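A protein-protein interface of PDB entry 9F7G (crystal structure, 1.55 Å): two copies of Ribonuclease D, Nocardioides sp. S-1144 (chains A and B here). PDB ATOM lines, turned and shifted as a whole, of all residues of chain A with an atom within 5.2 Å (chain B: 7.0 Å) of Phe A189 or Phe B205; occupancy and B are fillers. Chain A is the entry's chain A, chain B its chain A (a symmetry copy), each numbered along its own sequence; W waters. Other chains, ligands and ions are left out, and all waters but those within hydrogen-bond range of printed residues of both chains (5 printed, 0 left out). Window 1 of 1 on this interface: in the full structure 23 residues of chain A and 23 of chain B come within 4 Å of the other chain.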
ATOM      1  N   HIS A  82     -11.005  12.204  26.801  1.00  0.00           N
ATOM      2  CA  HIS A  82      -9.689  12.469  26.239  1.00  0.00           C
ATOM      3  C   HIS A  82      -9.779  12.657  24.725  1.00  0.00           C
ATOM      4  O   HIS A  82      -9.174  11.931  23.919  1.00  0.00           O
ATOM      5  CB  HIS A  82      -8.659  11.411  26.617  1.00  0.00           C
ATOM      6  CG  HIS A  82      -7.270  11.897  26.402  1.00  0.00           C
ATOM      7  ND1 HIS A  82      -6.262  11.129  25.860  1.00  0.00           N
ATOM      8  CD2 HIS A  82      -6.738  13.122  26.614  1.00  0.00           C
ATOM      9  CE1 HIS A  82      -5.160  11.856  25.771  1.00  0.00           C
ATOM     10  NE2 HIS A  82      -5.429  13.071  26.207  1.00  0.00           N
ATOM     11  N   PRO A  84      -8.283  14.796  22.830  1.00  0.00           N
ATOM     12  CA  PRO A  84      -7.039  14.956  22.057  1.00  0.00           C
ATOM     13  C   PRO A  84      -6.565  13.683  21.386  1.00  0.00           C
ATOM     14  O   PRO A  84      -6.174  13.721  20.211  1.00  0.00           O
ATOM     15  CB  PRO A  84      -6.048  15.462  23.116  1.00  0.00           C
ATOM     16  CG  PRO A  84      -6.913  16.281  24.025  1.00  0.00           C
ATOM     17  CD  PRO A  84      -8.164  15.446  24.156  1.00  0.00           C
ATOM     18  N   ILE A 106     -10.486  16.687  29.957  1.00  0.00           N
ATOM     19  CA  ILE A 106     -10.108  18.084  30.124  1.00  0.00           C
ATOM     20  C   ILE A 106     -10.966  18.739  31.197  1.00  0.00           C
ATOM     21  O   ILE A 106     -10.461  19.497  32.033  1.00  0.00           O
ATOM     22  CB  ILE A 106     -10.202  18.825  28.781  1.00  0.00           C
ATOM     23  CG1 ILE A 106      -9.076  18.350  27.852  1.00  0.00           C
ATOM     24  CG2 ILE A 106     -10.166  20.351  28.985  1.00  0.00           C
ATOM     25  CD1 ILE A 106      -9.258  18.787  26.406  1.00  0.00           C
ATOM     26  N   GLU A 184     -14.795  25.589  28.480  1.00  0.00           N
ATOM     27  CA  GLU A 184     -15.233  25.807  27.105  1.00  0.00           C
ATOM     28  C   GLU A 184     -14.149  26.481  26.271  1.00  0.00           C
ATOM     29  O   GLU A 184     -14.061  26.242  25.059  1.00  0.00           O
ATOM     30  CB  GLU A 184     -16.528  26.625  27.086  1.00  0.00           C
ATOM     31  CG  GLU A 184     -17.727  25.899  27.698  1.00  0.00           C
ATOM     32  CD  GLU A 184     -18.502  25.082  26.692  1.00  0.00           C
ATOM     33  OE1 GLU A 184     -18.071  25.002  25.520  1.00  0.00           O
ATOM     34  OE2 GLU A 184     -19.557  24.529  27.073  1.00  0.00           O
ATOM     35  N   ASN A 185     -13.316  27.328  26.887  1.00  0.00           N
ATOM     36  CA  ASN A 185     -12.204  27.900  26.134  1.00  0.00           C
ATOM     37  C   ASN A 185     -11.170  26.842  25.772  1.00  0.00           C
ATOM     38  O   ASN A 185     -10.568  26.910  24.690  1.00  0.00           O
ATOM     39  CB  ASN A 185     -11.567  29.050  26.922  1.00  0.00           C
ATOM     40  CG  ASN A 185     -12.406  30.308  26.875  1.00  0.00           C
ATOM     41  OD1 ASN A 185     -13.081  30.565  25.878  1.00  0.00           O
ATOM     42  ND2 ASN A 185     -12.379  31.094  27.949  1.00  0.00           N
ATOM     43  N   ALA A 186     -10.967  25.844  26.635  1.00  0.00           N
ATOM     44  CA  ALA A 186     -10.111  24.725  26.252  1.00  0.00           C
ATOM     45  C   ALA A 186     -10.724  23.949  25.090  1.00  0.00           C
ATOM     46  O   ALA A 186     -10.025  23.593  24.132  1.00  0.00           O
ATOM     47  CB  ALA A 186      -9.869  23.802  27.448  1.00  0.00           C
ATOM     48  N   TYR A 187     -12.038  23.710  25.142  1.00  0.00           N
ATOM     49  CA  TYR A 187     -12.702  22.968  24.070  1.00  0.00           C
ATOM     50  C   TYR A 187     -12.582  23.694  22.737  1.00  0.00           C
ATOM     51  O   TYR A 187     -12.380  23.063  21.691  1.00  0.00           O
ATOM     52  CB  TYR A 187     -14.178  22.770  24.398  1.00  0.00           C
ATOM     53  CG  TYR A 187     -14.499  21.864  25.567  1.00  0.00           C
ATOM     54  CD1 TYR A 187     -13.530  21.062  26.165  1.00  0.00           C
ATOM     55  CD2 TYR A 187     -15.797  21.809  26.071  1.00  0.00           C
ATOM     56  CE1 TYR A 187     -13.855  20.226  27.244  1.00  0.00           C
ATOM     57  CE2 TYR A 187     -16.129  20.989  27.138  1.00  0.00           C
ATOM     58  CZ  TYR A 187     -15.166  20.189  27.709  1.00  0.00           C
ATOM     59  OH  TYR A 187     -15.528  19.371  28.756  1.00  0.00           O
ATOM     60  N   SER A 188     -12.730  25.023  22.753  1.00  0.00           N
ATOM     61  CA  SER A 188     -12.675  25.808  21.524  1.00  0.00           C
ATOM     62  C   SER A 188     -11.289  25.805  20.895  1.00  0.00           C
ATOM     63  O   SER A 188     -11.165  26.085  19.698  1.00  0.00           O
ATOM     64  CB  SER A 188     -13.103  27.247  21.802  1.00  0.00           C
ATOM     65  OG  SER A 188     -14.472  27.292  22.155  1.00  0.00           O
ATOM     66  N   PHE A 189     -10.250  25.513  21.677  1.00  0.00           N
ATOM     67  CA  PHE A 189      -8.898  25.416  21.144  1.00  0.00           C
ATOM     68  C   PHE A 189      -8.606  24.046  20.531  1.00  0.00           C
ATOM     69  O   PHE A 189      -7.655  23.919  19.760  1.00  0.00           O
ATOM     70  CB  PHE A 189      -7.897  25.759  22.260  1.00  0.00           C
ATOM     71  CG  PHE A 189      -6.454  25.654  21.843  1.00  0.00           C
ATOM     72  CD1 PHE A 189      -5.926  26.515  20.883  1.00  0.00           C
ATOM     73  CD2 PHE A 189      -5.622  24.693  22.410  1.00  0.00           C
ATOM     74  CE1 PHE A 189      -4.592  26.408  20.486  1.00  0.00           C
ATOM     75  CE2 PHE A 189      -4.287  24.586  22.021  1.00  0.00           C
ATOM     76  CZ  PHE A 189      -3.773  25.447  21.060  1.00  0.00           C
ATOM     77  N   LEU A 190      -9.420  23.031  20.818  1.00  0.00           N
ATOM     78  CA  LEU A 190      -9.114  21.688  20.322  1.00  0.00           C
ATOM     79  C   LEU A 190      -8.935  21.604  18.806  1.00  0.00           C
ATOM     80  O   LEU A 190      -7.987  20.926  18.367  1.00  0.00           O
ATOM     81  CB  LEU A 190     -10.188  20.703  20.800  1.00  0.00           C
ATOM     82  CG  LEU A 190     -10.102  20.281  22.272  1.00  0.00           C
ATOM     83  CD1 LEU A 190     -11.352  19.502  22.644  1.00  0.00           C
ATOM     84  CD2 LEU A 190      -8.839  19.448  22.537  1.00  0.00           C
ATOM     85  N   PRO A 191      -9.777  22.222  17.964  1.00  0.00           N
ATOM     86  CA  PRO A 191      -9.508  22.155  16.514  1.00  0.00           C
ATOM     87  C   PRO A 191      -8.196  22.810  16.126  1.00  0.00           C
ATOM     88  O   PRO A 191      -7.524  22.355  15.189  1.00  0.00           O
ATOM     89  CB  PRO A 191     -10.708  22.892  15.897  1.00  0.00           C
ATOM     90  CG  PRO A 191     -11.780  22.813  16.927  1.00  0.00           C
ATOM     91  CD  PRO A 191     -11.068  22.870  18.249  1.00  0.00           C
ATOM     92  N   VAL A 192      -7.810  23.878  16.821  1.00  0.00           N
ATOM     93  CA  VAL A 192      -6.535  24.524  16.537  1.00  0.00           C
ATOM     94  C   VAL A 192      -5.391  23.628  16.984  1.00  0.00           C
ATOM     95  O   VAL A 192      -4.404  23.438  16.261  1.00  0.00           O
ATOM     96  CB  VAL A 192      -6.483  25.896  17.234  1.00  0.00           C
ATOM     97  CG1 VAL A 192      -5.220  26.652  16.849  1.00  0.00           C
ATOM     98  CG2 VAL A 192      -7.740  26.697  16.916  1.00  0.00           C
ATOM     99  N   TRP A 193      -5.512  23.080  18.194  1.00  0.00           N
ATOM    100  CA  TRP A 193      -4.509  22.173  18.734  1.00  0.00           C
ATOM    101  C   TRP A 193      -4.214  21.028  17.774  1.00  0.00           C
ATOM    102  O   TRP A 193      -3.053  20.714  17.510  1.00  0.00           O
ATOM    103  CB  TRP A 193      -4.978  21.643  20.092  1.00  0.00           C
ATOM    104  CG  TRP A 193      -4.056  20.619  20.677  1.00  0.00           C
ATOM    105  CD1 TRP A 193      -2.964  20.854  21.459  1.00  0.00           C
ATOM    106  CD2 TRP A 193      -4.143  19.195  20.526  1.00  0.00           C
ATOM    107  NE1 TRP A 193      -2.368  19.666  21.813  1.00  0.00           N
ATOM    108  CE2 TRP A 193      -3.068  18.634  21.243  1.00  0.00           C
ATOM    109  CE3 TRP A 193      -5.029  18.340  19.851  1.00  0.00           C
ATOM    110  CZ2 TRP A 193      -2.853  17.258  21.310  1.00  0.00           C
ATOM    111  CZ3 TRP A 193      -4.810  16.974  19.917  1.00  0.00           C
ATOM    112  CH2 TRP A 193      -3.734  16.448  20.643  1.00  0.00           C
ATOM    113  N   VAL A 194      -5.254  20.402  17.218  1.00  0.00           N
ATOM    114  CA  VAL A 194      -4.983  19.209  16.425  1.00  0.00           C
ATOM    115  C   VAL A 194      -4.365  19.581  15.080  1.00  0.00           C
ATOM    116  O   VAL A 194      -3.528  18.839  14.551  1.00  0.00           O
ATOM    117  CB  VAL A 194      -6.258  18.357  16.269  1.00  0.00           C
ATOM    118  CG1 VAL A 194      -7.245  19.014  15.342  1.00  0.00           C
ATOM    119  CG2 VAL A 194      -5.901  16.958  15.776  1.00  0.00           C
ATOM    120  N   LEU A 196      -2.300  22.103  14.657  1.00  0.00           N
ATOM    121  CA  LEU A 196      -0.904  22.319  15.019  1.00  0.00           C
ATOM    122  C   LEU A 196      -0.160  20.995  15.176  1.00  0.00           C
ATOM    123  O   LEU A 196       0.982  20.863  14.720  1.00  0.00           O
ATOM    124  CB  LEU A 196      -0.819  23.158  16.297  1.00  0.00           C
ATOM    125  CG  LEU A 196      -1.262  24.611  16.107  1.00  0.00           C
ATOM    126  CD1 LEU A 196      -1.529  25.255  17.460  1.00  0.00           C
ATOM    127  CD2 LEU A 196      -0.200  25.386  15.333  1.00  0.00           C
ATOM    128  N   VAL A 204       1.928  24.986  21.185  1.00  0.00           N
ATOM    129  CA  VAL A 204       2.089  26.349  20.688  1.00  0.00           C
ATOM    130  C   VAL A 204       2.402  27.319  21.822  1.00  0.00           C
ATOM    131  O   VAL A 204       2.865  28.438  21.565  1.00  0.00           O
ATOM    132  CB  VAL A 204       0.828  26.766  19.902  1.00  0.00           C
ATOM    133  CG1 VAL A 204      -0.318  27.150  20.843  1.00  0.00           C
ATOM    134  CG2 VAL A 204       1.132  27.881  18.893  1.00  0.00           C
ATOM    135  N   PHE A 205       2.186  26.913  23.077  1.00  0.00           N
ATOM    136  CA  PHE A 205       2.460  27.781  24.220  1.00  0.00           C
ATOM    137  C   PHE A 205       3.878  27.633  24.745  1.00  0.00           C
ATOM    138  O   PHE A 205       4.320  28.466  25.546  1.00  0.00           O
ATOM    139  CB  PHE A 205       1.428  27.509  25.325  1.00  0.00           C
ATOM    140  CG  PHE A 205       0.021  27.594  24.827  1.00  0.00           C
ATOM    141  CD1 PHE A 205      -0.545  28.820  24.525  1.00  0.00           C
ATOM    142  CD2 PHE A 205      -0.712  26.446  24.573  1.00  0.00           C
ATOM    143  CE1 PHE A 205      -1.837  28.900  24.018  1.00  0.00           C
ATOM    144  CE2 PHE A 205      -1.998  26.523  24.075  1.00  0.00           C
ATOM    145  CZ  PHE A 205      -2.558  27.751  23.792  1.00  0.00           C
ATOM    146  N   ILE B 106       2.430  33.261  19.058  1.00  0.00           N
ATOM    147  CA  ILE B 106       1.389  32.288  18.752  1.00  0.00           C
ATOM    148  C   ILE B 106       0.801  32.559  17.375  1.00  0.00           C
ATOM    149  O   ILE B 106       0.565  31.629  16.595  1.00  0.00           O
ATOM    150  CB  ILE B 106       0.313  32.297  19.849  1.00  0.00           C
ATOM    151  CG1 ILE B 106       0.883  31.685  21.135  1.00  0.00           C
ATOM    152  CG2 ILE B 106      -0.959  31.563  19.384  1.00  0.00           C
ATOM    153  CD1 ILE B 106       0.011  31.924  22.359  1.00  0.00           C
ATOM    154  N   VAL B 110       0.782  29.819  14.352  1.00  0.00           N
ATOM    155  CA  VAL B 110      -0.421  29.315  13.690  1.00  0.00           C
ATOM    156  C   VAL B 110      -0.371  29.618  12.195  1.00  0.00           C
ATOM    157  O   VAL B 110      -0.812  28.807  11.367  1.00  0.00           O
ATOM    158  CB  VAL B 110      -1.682  29.898  14.352  1.00  0.00           C
ATOM    159  CG1 VAL B 110      -2.943  29.528  13.551  1.00  0.00           C
ATOM    160  CG2 VAL B 110      -1.795  29.417  15.797  1.00  0.00           C
ATOM    161  N   ALA B 182      -8.918  30.855  14.492  1.00  0.00           N
ATOM    162  CA  ALA B 182      -8.063  29.873  15.149  1.00  0.00           C
ATOM    163  C   ALA B 182      -7.107  30.551  16.116  1.00  0.00           C
ATOM    164  O   ALA B 182      -6.948  30.116  17.263  1.00  0.00           O
ATOM    165  CB  ALA B 182      -7.280  29.074  14.112  1.00  0.00           C
ATOM    166  N   VAL B 183      -6.441  31.613  15.658  1.00  0.00           N
ATOM    167  CA  VAL B 183      -5.526  32.344  16.533  1.00  0.00           C
ATOM    168  C   VAL B 183      -6.263  32.886  17.750  1.00  0.00           C
ATOM    169  O   VAL B 183      -5.775  32.786  18.884  1.00  0.00           O
ATOM    170  CB  VAL B 183      -4.827  33.463  15.746  1.00  0.00           C
ATOM    171  CG1 VAL B 183      -4.040  34.355  16.689  1.00  0.00           C
ATOM    172  CG2 VAL B 183      -3.902  32.871  14.711  1.00  0.00           C
ATOM    173  N   ASN B 185      -8.892  31.687  19.147  1.00  0.00           N
ATOM    174  CA  ASN B 185      -9.197  30.598  20.070  1.00  0.00           C
ATOM    175  C   ASN B 185      -7.983  30.215  20.906  1.00  0.00           C
ATOM    176  O   ASN B 185      -8.131  29.857  22.084  1.00  0.00           O
ATOM    177  CB  ASN B 185      -9.743  29.389  19.301  1.00  0.00           C
ATOM    178  CG  ASN B 185     -11.179  29.590  18.869  1.00  0.00           C
ATOM    179  OD1 ASN B 185     -11.947  30.257  19.561  1.00  0.00           O
ATOM    180  ND2 ASN B 185     -11.550  29.024  17.722  1.00  0.00           N
ATOM    181  N   ALA B 186      -6.778  30.312  20.339  1.00  0.00           N
ATOM    182  CA  ALA B 186      -5.583  30.116  21.155  1.00  0.00           C
ATOM    183  C   ALA B 186      -5.466  31.210  22.212  1.00  0.00           C
ATOM    184  O   ALA B 186      -5.168  30.927  23.380  1.00  0.00           O
ATOM    185  CB  ALA B 186      -4.333  30.083  20.273  1.00  0.00           C
ATOM    186  N   TYR B 187      -5.732  32.462  21.827  1.00  0.00           N
ATOM    187  CA  TYR B 187      -5.638  33.569  22.779  1.00  0.00           C
ATOM    188  C   TYR B 187      -6.618  33.395  23.931  1.00  0.00           C
ATOM    189  O   TYR B 187      -6.290  33.685  25.088  1.00  0.00           O
ATOM    190  CB  TYR B 187      -5.922  34.894  22.080  1.00  0.00           C
ATOM    191  CG  TYR B 187      -4.906  35.355  21.058  1.00  0.00           C
ATOM    192  CD1 TYR B 187      -3.663  34.740  20.926  1.00  0.00           C
ATOM    193  CD2 TYR B 187      -5.197  36.429  20.219  1.00  0.00           C
ATOM    194  CE1 TYR B 187      -2.736  35.190  19.973  1.00  0.00           C
ATOM    195  CE2 TYR B 187      -4.290  36.880  19.273  1.00  0.00           C
ATOM    196  CZ  TYR B 187      -3.060  36.275  19.164  1.00  0.00           C
ATOM    197  OH  TYR B 187      -2.171  36.755  18.228  1.00  0.00           O
ATOM    198  N   SER B 188      -7.840  32.943  23.626  1.00  0.00           N
ATOM    199  CA  SER B 188      -8.867  32.781  24.650  1.00  0.00           C
ATOM    200  C   SER B 188      -8.527  31.678  25.643  1.00  0.00           C
ATOM    201  O   SER B 188      -9.074  31.668  26.751  1.00  0.00           O
ATOM    202  CB  SER B 188     -10.214  32.478  23.998  1.00  0.00           C
ATOM    203  OG  SER B 188     -10.665  33.599  23.262  1.00  0.00           O
ATOM    204  N   PHE B 189      -7.654  30.744  25.264  1.00  0.00           N
ATOM    205  CA  PHE B 189      -7.217  29.695  26.174  1.00  0.00           C
ATOM    206  C   PHE B 189      -6.078  30.149  27.089  1.00  0.00           C
ATOM    207  O   PHE B 189      -5.834  29.509  28.111  1.00  0.00           O
ATOM    208  CB  PHE B 189      -6.821  28.456  25.352  1.00  0.00           C
ATOM    209  CG  PHE B 189      -6.308  27.309  26.182  1.00  0.00           C
ATOM    210  CD1 PHE B 189      -7.146  26.647  27.076  1.00  0.00           C
ATOM    211  CD2 PHE B 189      -4.986  26.890  26.069  1.00  0.00           C
ATOM    212  CE1 PHE B 189      -6.668  25.592  27.855  1.00  0.00           C
ATOM    213  CE2 PHE B 189      -4.504  25.833  26.840  1.00  0.00           C
ATOM    214  CZ  PHE B 189      -5.348  25.183  27.732  1.00  0.00           C
ATOM    215  N   TRP B 193      -4.745  28.278  30.358  1.00  0.00           N
ATOM    216  CA  TRP B 193      -3.414  27.689  30.311  1.00  0.00           C
ATOM    217  C   TRP B 193      -2.573  28.107  31.510  1.00  0.00           C
ATOM    218  O   TRP B 193      -1.938  27.270  32.152  1.00  0.00           O
ATOM    219  CB  TRP B 193      -2.729  28.081  28.998  1.00  0.00           C
ATOM    220  CG  TRP B 193      -1.313  27.607  28.905  1.00  0.00           C
ATOM    221  CD1 TRP B 193      -0.884  26.398  28.443  1.00  0.00           C
ATOM    222  CD2 TRP B 193      -0.135  28.332  29.286  1.00  0.00           C
ATOM    223  NE1 TRP B 193       0.488  26.325  28.505  1.00  0.00           N
ATOM    224  CE2 TRP B 193       0.970  27.496  29.028  1.00  0.00           C
ATOM    225  CE3 TRP B 193       0.091  29.610  29.822  1.00  0.00           C
ATOM    226  CZ2 TRP B 193       2.281  27.894  29.283  1.00  0.00           C
ATOM    227  CZ3 TRP B 193       1.395  30.000  30.077  1.00  0.00           C
ATOM    228  CH2 TRP B 193       2.472  29.147  29.805  1.00  0.00           C
ATOM    229  N   LEU B 196      -3.706  26.531  34.791  1.00  0.00           N
ATOM    230  CA  LEU B 196      -3.268  25.140  34.815  1.00  0.00           C
ATOM    231  C   LEU B 196      -1.778  25.033  35.129  1.00  0.00           C
ATOM    232  O   LEU B 196      -1.365  24.169  35.912  1.00  0.00           O
ATOM    233  CB  LEU B 196      -3.605  24.463  33.484  1.00  0.00           C
ATOM    234  CG  LEU B 196      -5.105  24.255  33.265  1.00  0.00           C
ATOM    235  CD1 LEU B 196      -5.381  23.958  31.797  1.00  0.00           C
ATOM    236  CD2 LEU B 196      -5.615  23.125  34.155  1.00  0.00           C
ATOM    237  N   ILE B 201      -0.595  21.425  35.975  1.00  0.00           N
ATOM    238  CA  ILE B 201      -0.935  20.773  34.710  1.00  0.00           C
ATOM    239  C   ILE B 201      -0.148  21.484  33.616  1.00  0.00           C
ATOM    240  O   ILE B 201      -0.472  22.616  33.244  1.00  0.00           O
ATOM    241  CB  ILE B 201      -2.442  20.808  34.421  1.00  0.00           C
ATOM    242  CG1 ILE B 201      -3.228  19.988  35.453  1.00  0.00           C
ATOM    243  CG2 ILE B 201      -2.729  20.314  32.995  1.00  0.00           C
ATOM    244  CD1 ILE B 201      -3.252  18.530  35.184  1.00  0.00           C
ATOM    245  N   GLU B 202       0.885  20.817  33.094  1.00  0.00           N
ATOM    246  CA  GLU B 202       1.766  21.436  32.108  1.00  0.00           C
ATOM    247  C   GLU B 202       1.167  21.435  30.705  1.00  0.00           C
ATOM    248  O   GLU B 202       1.490  22.312  29.898  1.00  0.00           O
ATOM    249  CB  GLU B 202       3.113  20.722  32.100  1.00  0.00           C
ATOM    250  CG  GLU B 202       3.858  20.852  33.412  1.00  0.00           C
ATOM    251  CD  GLU B 202       5.323  20.514  33.287  1.00  0.00           C
ATOM    252  OE1 GLU B 202       5.642  19.319  33.108  1.00  0.00           O
ATOM    253  OE2 GLU B 202       6.155  21.447  33.357  1.00  0.00           O
ATOM    254  N   ASP B 203       0.300  20.468  30.396  1.00  0.00           N
ATOM    255  CA  ASP B 203      -0.354  20.409  29.090  1.00  0.00           C
ATOM    256  C   ASP B 203      -1.645  19.623  29.301  1.00  0.00           C
ATOM    257  O   ASP B 203      -1.605  18.396  29.436  1.00  0.00           O
ATOM    258  CB  ASP B 203       0.542  19.751  28.055  1.00  0.00           C
ATOM    259  CG  ASP B 203      -0.092  19.688  26.679  1.00  0.00           C
ATOM    260  OD1 ASP B 203      -1.229  20.186  26.512  1.00  0.00           O
ATOM    261  OD2 ASP B 203       0.566  19.136  25.758  1.00  0.00           O
ATOM    262  N   VAL B 204      -2.770  20.340  29.351  1.00  0.00           N
ATOM    263  CA  VAL B 204      -4.054  19.697  29.611  1.00  0.00           C
ATOM    264  C   VAL B 204      -4.463  18.788  28.458  1.00  0.00           C
ATOM    265  O   VAL B 204      -5.349  17.940  28.626  1.00  0.00           O
ATOM    266  CB  VAL B 204      -5.121  20.771  29.907  1.00  0.00           C
ATOM    267  CG1 VAL B 204      -5.616  21.439  28.620  1.00  0.00           C
ATOM    268  CG2 VAL B 204      -6.282  20.205  30.735  1.00  0.00           C
ATOM    269  N   PHE B 205      -3.822  18.922  27.292  1.00  0.00           N
ATOM    270  CA  PHE B 205      -4.153  18.090  26.137  1.00  0.00           C
ATOM    271  C   PHE B 205      -3.339  16.808  26.082  1.00  0.00           C
ATOM    272  O   PHE B 205      -3.675  15.907  25.303  1.00  0.00           O
ATOM    273  CB  PHE B 205      -3.980  18.913  24.851  1.00  0.00           C
ATOM    274  CG  PHE B 205      -4.727  20.207  24.895  1.00  0.00           C
ATOM    275  CD1 PHE B 205      -6.105  20.228  24.787  1.00  0.00           C
ATOM    276  CD2 PHE B 205      -4.063  21.400  25.135  1.00  0.00           C
ATOM    277  CE1 PHE B 205      -6.807  21.424  24.874  1.00  0.00           C
ATOM    278  CE2 PHE B 205      -4.757  22.591  25.215  1.00  0.00           C
ATOM    279  CZ  PHE B 205      -6.131  22.602  25.091  1.00  0.00           C
ATOM    280  N   ALA B 206      -2.300  16.695  26.905  1.00  0.00           N
ATOM    281  CA  ALA B 206      -1.561  15.451  27.017  1.00  0.00           C
ATOM    282  C   ALA B 206      -2.391  14.419  27.769  1.00  0.00           C
ATOM    283  O   ALA B 206      -3.327  14.755  28.502  1.00  0.00           O
ATOM    284  CB  ALA B 206      -0.242  15.685  27.746  1.00  0.00           C
ATOM    285  N   TYR B 207      -2.026  13.152  27.595  1.00  0.00           N
ATOM    286  CA  TYR B 207      -2.683  12.083  28.334  1.00  0.00           C
ATOM    287  C   TYR B 207      -2.631  12.346  29.843  1.00  0.00           C
ATOM    288  O   TYR B 207      -3.642  12.223  30.548  1.00  0.00           O
ATOM    289  CB  TYR B 207      -2.049  10.733  28.012  1.00  0.00           C
ATOM    290  CG  TYR B 207      -2.652   9.616  28.813  1.00  0.00           C
ATOM    291  CD1 TYR B 207      -3.925   9.152  28.533  1.00  0.00           C
ATOM    292  CD2 TYR B 207      -1.963   9.039  29.864  1.00  0.00           C
ATOM    293  CE1 TYR B 207      -4.493   8.141  29.276  1.00  0.00           C
ATOM    294  CE2 TYR B 207      -2.522   8.014  30.607  1.00  0.00           C
ATOM    295  CZ  TYR B 207      -3.790   7.575  30.310  1.00  0.00           C
ATOM    296  OH  TYR B 207      -4.352   6.565  31.056  1.00  0.00           O
ATOM    297  OXT TYR B 207      -1.583  12.710  30.379  1.00  0.00           O
HETATM  298  O   HOH W   1     -10.307  33.778  27.980  1.00  0.00           O
HETATM  299  O   HOH W   2     -10.545  29.149  23.135  1.00  0.00           O
HETATM  300  O   HOH W   3      -0.022  20.314  23.403  1.00  0.00           O
HETATM  301  O   HOH W   4     -13.129  26.023  17.795  1.00  0.00           O
HETATM  302  O   HOH W   5     -12.766  30.572  22.667  1.00  0.00           O
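Hydrophobic or aromatic side chains of chain B within 4 Å of the printed part of chain A: Ile B106, Ala B182, Ala B186, Phe B189, Trp B193, Phe B205 and Tyr B207.
Along chain B the printed residues that touch a printed residue of chain A span positions 106 to 207.
Among the printed residues, 20 pairs touch across the chains.
Ile A106 touches Phe B205, and with the chains exchanged Phe A205 touches Ile B106.
Ala A186 touches Phe B205, and with the chains exchanged Phe A205 touches Ala B186.
Phe A189 touches Phe B205, and with the chains exchanged Phe A205 touches Phe B189.
Trp A193 touches Phe B205, and with the chains exchanged Phe A205 touches Trp B193.
Of the 20 pairs that touch across the chains among the printed residues, 14 have their exchanged pair printed and touching as well.
The backbone carbonyl oxygen of Glu A184 lies within hydrogen-bond range of the side-chain hydroxyl of Ser A188 (3.1 Å).
The backbone NH (N) of Phe B205 sits at hydrogen-bond distance from the side-chain carboxylate (OD1) of Asp B203, 3.0 Å away.
Among the printed residues, merely in contact across the chains: His A82 with Ala B206, His A82 with Tyr B207, Pro A84 with Phe B205, Ile A106 with Val B204, Ile A106 with Phe B205, Asn A185 with Ser B188, Ala A186 with Phe B189, Ala A186 with Phe B205, Ser A188 with Asn B185, Phe A189 with Ala B186, Phe A189 with Phe B205, Leu A190 with Phe B205, Val A192 with Ala B182, Trp A193 with Phe B205, Val A204 with Ile B106, Phe A205 with Ile B106, Phe A205 with Ala B186, Phe A205 with Phe B189 and Phe A205 with Trp B193.
Glu A184 touches none of the printed residues of chain B.
Of the printed residues of chain B, Ala A186 touches Phe B189 (3.6 Å) and Phe B205 (3.95 Å).
Of chain B, only Ala B186 and Phe B205 come within 4 Å of Phe A189.
Printed residues of chain A within 4 Å of Ala B182: Val A192 (3.5 Å).
Ile B201 touches none of the printed residues of chain A.
Of the printed residues of chain A, Val B204 touches Ile A106.
Of the printed residues of chain A, Ala B206 touches His A82 (3.5 Å).
The nearest residue of chain B that does not touch Phe A189 is Asn B185 (4.1 Å).
The nearest printed residue of chain B that does not touch Pro A84 is Val B204 (5.1 Å).
Water W3 bridges the side-chain carboxylate (OD2) of Asp B203 (2.7 Å) and the indole nitrogen (NE1) of Trp A193 (2.9 Å).
Water W2 lies within hydrogen-bond range of O of Asn A185 (2.7 Å) and O of Asn B185 (2.7 Å).
Water W4 bridges the backbone carbonyl oxygen of Ser A188 (2.7 Å) and the side-chain amide nitrogen of Asn B185 (3.4 Å).
Water W1 lies within hydrogen-bond range of the backbone carbonyl oxygen (O) of Ser B188 (2.7 Å) and the side-chain amide nitrogen (ND2) of Asn A185 (3.4 Å).
Water W5 bridges OD1 of Asn A185 (3.2 Å) and OD1 of Asn B185 (3.2 Å).
A ring nitrogen (NE2) of His A82 is in hydrogen-bond range of the backbone carbonyl oxygen (O) of Phe B205 (3.5 Å).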
